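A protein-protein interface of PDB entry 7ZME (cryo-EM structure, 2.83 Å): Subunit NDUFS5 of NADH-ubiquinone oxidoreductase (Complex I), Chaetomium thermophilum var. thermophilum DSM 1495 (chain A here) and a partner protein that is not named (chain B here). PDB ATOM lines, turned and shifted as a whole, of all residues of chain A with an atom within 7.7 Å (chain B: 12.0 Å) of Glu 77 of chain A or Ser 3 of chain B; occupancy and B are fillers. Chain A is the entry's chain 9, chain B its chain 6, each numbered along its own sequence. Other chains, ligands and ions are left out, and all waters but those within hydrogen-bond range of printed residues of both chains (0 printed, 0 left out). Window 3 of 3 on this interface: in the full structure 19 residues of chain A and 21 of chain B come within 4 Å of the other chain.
Lys 74 of chain A touches Ser 3 of chain B (CE to CB, 3.8 Å). CD1 of Leu 8 of chain B touches CG1 of Val 100 of chain A (3.997 Å).
The side-chain carboxylate (OE2) of Glu 77 of chain A sits at hydrogen-bond distance from the backbone NH (N) of Ser 3 of chain B (2.9 Å). The backbone carbonyl oxygen (O) of Ser 3 of chain B sits at hydrogen-bond distance from the side-chain sulfur (SG) of Cys 102 of chain A, at 3.6 Å. O of Gln 4 of chain B is in hydrogen-bond range of NZ of Lys 74 of chain A, at 3.4 Å.
Hydrophobic or aromatic side chains of chain B that line the printed part of chain A: Leu 8. Of the 10 printed residues of chain A, 4 touch a printed residue of chain B. Printed residues of chain A that touch a printed residue of chain B: Lys 74, Glu 77, Val 100 and Cys 102. Hydrophobic or aromatic side chains of chain A that line the printed part of chain B: Val 100. Along chain A the printed residues that touch a printed residue of chain B span positions 74 to 102. Among the printed residues, no Asp or Glu carboxylate lies within 4 Å of a Lys or Arg side-chain nitrogen of the other chain.
Of the printed residues of chain B, Lys 74 of chain A touches Ser 3 and Gln 4. No residue of chain B comes within 4 Å of Leu 75 of chain A. No residue of chain B comes within 4 Å of Gln 76 of chain A. Of chain B, only Ser 3 comes within 4 Å of Glu 77 of chain A. No residue of chain B comes within 4 Å of Asn 78 of chain A. No residue of chain B comes within 4 Å of Pro 79 of chain A. Printed residues of chain B within 4 Å of Val 100 of chain A: Leu 8 (3.997 Å). Ser 3 of chain B touches just these residues of chain A: Lys 74 (3.8 Å), Glu 77 (2.9 Å) and Cys 102 (3.6 Å). Printed residues of chain A within 4 Å of Gln 4 of chain B: Lys 74. Ser 6 of chain B touches none of the printed residues of chain A. Printed residues of chain A within 4 Å of Leu 8 of chain B: Val 100 (3.997 Å). The nearest printed residue of chain B that does not touch Val 100 of chain A is Ser 6 of chain B (6.3 Å).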
ATOM      1  N   LYS A  74     -37.636 -17.094  15.272  1.00  0.00           N
ATOM      2  CA  LYS A  74     -36.247 -17.510  15.408  1.00  0.00           C
ATOM      3  C   LYS A  74     -35.301 -16.378  15.031  1.00  0.00           C
ATOM      4  O   LYS A  74     -35.571 -15.596  14.116  1.00  0.00           O
ATOM      5  CB  LYS A  74     -35.972 -18.735  14.536  1.00  0.00           C
ATOM      6  CG  LYS A  74     -34.971 -19.710  15.133  1.00  0.00           C
ATOM      7  CD  LYS A  74     -35.005 -21.045  14.408  1.00  0.00           C
ATOM      8  CE  LYS A  74     -34.229 -22.106  15.169  1.00  0.00           C
ATOM      9  NZ  LYS A  74     -34.388 -23.452  14.554  1.00  0.00           N
ATOM     10  N   LEU A  75     -34.184 -16.295  15.751  1.00  0.00           N
ATOM     11  CA  LEU A  75     -33.178 -15.283  15.459  1.00  0.00           C
ATOM     12  C   LEU A  75     -32.531 -15.557  14.109  1.00  0.00           C
ATOM     13  O   LEU A  75     -32.162 -16.694  13.800  1.00  0.00           O
ATOM     14  CB  LEU A  75     -32.120 -15.258  16.562  1.00  0.00           C
ATOM     15  CG  LEU A  75     -32.629 -15.015  17.983  1.00  0.00           C
ATOM     16  CD1 LEU A  75     -31.513 -15.220  18.995  1.00  0.00           C
ATOM     17  CD2 LEU A  75     -33.221 -13.619  18.109  1.00  0.00           C
ATOM     18  N   GLN A  76     -32.396 -14.508  13.303  1.00  0.00           N
ATOM     19  CA  GLN A  76     -31.825 -14.602  11.967  1.00  0.00           C
ATOM     20  C   GLN A  76     -30.565 -13.752  11.898  1.00  0.00           C
ATOM     21  O   GLN A  76     -30.571 -12.590  12.318  1.00  0.00           O
ATOM     22  CB  GLN A  76     -32.839 -14.153  10.913  1.00  0.00           C
ATOM     23  CG  GLN A  76     -32.404 -14.400   9.481  1.00  0.00           C
ATOM     24  CD  GLN A  76     -31.574 -13.262   8.925  1.00  0.00           C
ATOM     25  OE1 GLN A  76     -31.758 -12.104   9.298  1.00  0.00           O
ATOM     26  NE2 GLN A  76     -30.645 -13.589   8.041  1.00  0.00           N
ATOM     27  N   GLU A  77     -29.489 -14.331  11.368  1.00  0.00           N
ATOM     28  CA  GLU A  77     -28.208 -13.644  11.251  1.00  0.00           C
ATOM     29  C   GLU A  77     -27.746 -13.483   9.809  1.00  0.00           C
ATOM     30  O   GLU A  77     -27.323 -12.391   9.419  1.00  0.00           O
ATOM     31  CB  GLU A  77     -27.138 -14.382  12.077  1.00  0.00           C
ATOM     32  CG  GLU A  77     -26.889 -15.834  11.680  1.00  0.00           C
ATOM     33  CD  GLU A  77     -27.831 -16.805  12.368  1.00  0.00           C
ATOM     34  OE1 GLU A  77     -28.856 -16.356  12.921  1.00  0.00           O
ATOM     35  OE2 GLU A  77     -27.545 -18.021  12.355  1.00  0.00           O
ATOM     36  N   ASN A  78     -27.825 -14.539   9.001  1.00  0.00           N
ATOM     37  CA  ASN A  78     -27.402 -14.489   7.606  1.00  0.00           C
ATOM     38  C   ASN A  78     -28.099 -15.588   6.814  1.00  0.00           C
ATOM     39  O   ASN A  78     -27.980 -16.771   7.155  1.00  0.00           O
ATOM     40  CB  ASN A  78     -25.884 -14.633   7.492  1.00  0.00           C
ATOM     41  CG  ASN A  78     -25.168 -13.296   7.488  1.00  0.00           C
ATOM     42  OD1 ASN A  78     -25.446 -12.434   6.655  1.00  0.00           O
ATOM     43  ND2 ASN A  78     -24.243 -13.117   8.423  1.00  0.00           N
ATOM     44  N   PRO A  79     -28.826 -15.244   5.756  1.00  0.00           N
ATOM     45  CA  PRO A  79     -29.518 -16.263   4.976  1.00  0.00           C
ATOM     46  C   PRO A  79     -28.632 -16.790   3.863  1.00  0.00           C
ATOM     47  O   PRO A  79     -27.955 -16.013   3.173  1.00  0.00           O
ATOM     48  CB  PRO A  79     -30.727 -15.503   4.415  1.00  0.00           C
ATOM     49  CG  PRO A  79     -30.219 -14.099   4.244  1.00  0.00           C
ATOM     50  CD  PRO A  79     -29.117 -13.884   5.268  1.00  0.00           C
ATOM     51  N   LYS A  99     -20.760 -23.570   4.700  1.00  0.00           N
ATOM     52  CA  LYS A  99     -21.634 -22.460   5.068  1.00  0.00           C
ATOM     53  C   LYS A  99     -23.091 -22.901   5.137  1.00  0.00           C
ATOM     54  O   LYS A  99     -23.849 -22.426   5.990  1.00  0.00           O
ATOM     55  CB  LYS A  99     -21.466 -21.308   4.078  1.00  0.00           C
ATOM     56  CG  LYS A  99     -22.341 -20.103   4.375  1.00  0.00           C
ATOM     57  CD  LYS A  99     -22.036 -19.526   5.747  1.00  0.00           C
ATOM     58  CE  LYS A  99     -23.090 -18.516   6.167  1.00  0.00           C
ATOM     59  NZ  LYS A  99     -24.437 -19.137   6.293  1.00  0.00           N
ATOM     60  N   VAL A 100     -23.501 -23.807   4.246  1.00  0.00           N
ATOM     61  CA  VAL A 100     -24.858 -24.341   4.268  1.00  0.00           C
ATOM     62  C   VAL A 100     -25.178 -25.069   5.564  1.00  0.00           C
ATOM     63  O   VAL A 100     -26.327 -25.040   6.017  1.00  0.00           O
ATOM     64  CB  VAL A 100     -25.069 -25.279   3.060  1.00  0.00           C
ATOM     65  CG1 VAL A 100     -26.429 -25.960   3.120  1.00  0.00           C
ATOM     66  CG2 VAL A 100     -24.922 -24.509   1.760  1.00  0.00           C
ATOM     67  N   HIS A 101     -24.183 -25.691   6.193  1.00  0.00           N
ATOM     68  CA  HIS A 101     -24.397 -26.499   7.385  1.00  0.00           C
ATOM     69  C   HIS A 101     -24.062 -25.755   8.670  1.00  0.00           C
ATOM     70  O   HIS A 101     -24.085 -26.361   9.747  1.00  0.00           O
ATOM     71  CB  HIS A 101     -23.573 -27.782   7.295  1.00  0.00           C
ATOM     72  CG  HIS A 101     -24.068 -28.737   6.256  1.00  0.00           C
ATOM     73  ND1 HIS A 101     -25.310 -28.622   5.673  1.00  0.00           N
ATOM     74  CD2 HIS A 101     -23.485 -29.820   5.691  1.00  0.00           C
ATOM     75  CE1 HIS A 101     -25.473 -29.595   4.796  1.00  0.00           C
ATOM     76  NE2 HIS A 101     -24.381 -30.335   4.787  1.00  0.00           N
ATOM     77  N   CYS A 102     -23.753 -24.459   8.583  1.00  0.00           N
ATOM     78  CA  CYS A 102     -23.384 -23.649   9.746  1.00  0.00           C
ATOM     79  C   CYS A 102     -22.205 -24.265  10.496  1.00  0.00           C
ATOM     80  O   CYS A 102     -22.147 -24.243  11.728  1.00  0.00           O
ATOM     81  CB  CYS A 102     -24.577 -23.442  10.682  1.00  0.00           C
ATOM     82  SG  CYS A 102     -25.758 -22.191  10.123  1.00  0.00           S
ATOM     83  N   SER B   3     -29.000 -19.741  14.164  1.00  0.00           N
ATOM     84  CA  SER B   3     -29.121 -21.112  14.643  1.00  0.00           C
ATOM     85  C   SER B   3     -28.964 -22.105  13.497  1.00  0.00           C
ATOM     86  O   SER B   3     -27.860 -22.324  13.001  1.00  0.00           O
ATOM     87  CB  SER B   3     -30.468 -21.319  15.341  1.00  0.00           C
ATOM     88  N   GLN B   4     -30.079 -22.706  13.080  1.00  0.00           N
ATOM     89  CA  GLN B   4     -30.056 -23.678  11.994  1.00  0.00           C
ATOM     90  C   GLN B   4     -31.429 -23.811  11.348  1.00  0.00           C
ATOM     91  O   GLN B   4     -32.375 -24.289  11.982  1.00  0.00           O
ATOM     92  CB  GLN B   4     -29.579 -25.039  12.505  1.00  0.00           C
ATOM     93  N   ILE B   5     -31.548 -23.411  10.079  1.00  0.00           N
ATOM     94  CA  ILE B   5     -32.842 -23.619   9.361  1.00  0.00           C
ATOM     95  C   ILE B   5     -33.010 -25.123   9.151  1.00  0.00           C
ATOM     96  O   ILE B   5     -33.927 -25.686   9.785  1.00  0.00           O
ATOM     97  CB  ILE B   5     -32.847 -22.866   8.017  1.00  0.00           C
ATOM     98  N   SER B   6     -32.227 -25.713   8.242  1.00  0.00           N
ATOM     99  CA  SER B   6     -32.238 -27.175   7.956  1.00  0.00           C
ATOM    100  C   SER B   6     -33.295 -27.544   6.914  1.00  0.00           C
ATOM    101  O   SER B   6     -33.158 -28.617   6.314  1.00  0.00           O
ATOM    102  CB  SER B   6     -32.290 -28.045   9.189  1.00  0.00           C
ATOM    103  OG  SER B   6     -31.093 -27.922   9.941  1.00  0.00           O
ATOM    104  N   LEU B   7     -34.252 -26.663   6.642  1.00  0.00           N
ATOM    105  CA  LEU B   7     -35.234 -26.933   5.559  1.00  0.00           C
ATOM    106  C   LEU B   7     -35.038 -25.840   4.518  1.00  0.00           C
ATOM    107  O   LEU B   7     -35.379 -24.687   4.814  1.00  0.00           O
ATOM    108  CB  LEU B   7     -36.664 -26.976   6.106  1.00  0.00           C
ATOM    109  CG  LEU B   7     -37.188 -28.366   6.456  1.00  0.00           C
ATOM    110  CD1 LEU B   7     -38.673 -28.310   6.766  1.00  0.00           C
ATOM    111  CD2 LEU B   7     -36.922 -29.343   5.323  1.00  0.00           C
ATOM    112  N   LEU B   8     -34.500 -26.192   3.352  1.00  0.00           N
ATOM    113  CA  LEU B   8     -34.139 -25.127   2.388  1.00  0.00           C
ATOM    114  C   LEU B   8     -35.023 -25.179   1.145  1.00  0.00           C
ATOM    115  O   LEU B   8     -35.046 -26.226   0.480  1.00  0.00           O
ATOM    116  CB  LEU B   8     -32.660 -25.287   2.037  1.00  0.00           C
ATOM    117  CG  LEU B   8     -31.734 -25.570   3.218  1.00  0.00           C
ATOM    118  CD1 LEU B   8     -30.405 -26.137   2.749  1.00  0.00           C
ATOM    119  CD2 LEU B   8     -31.522 -24.322   4.057  1.00  0.00           C
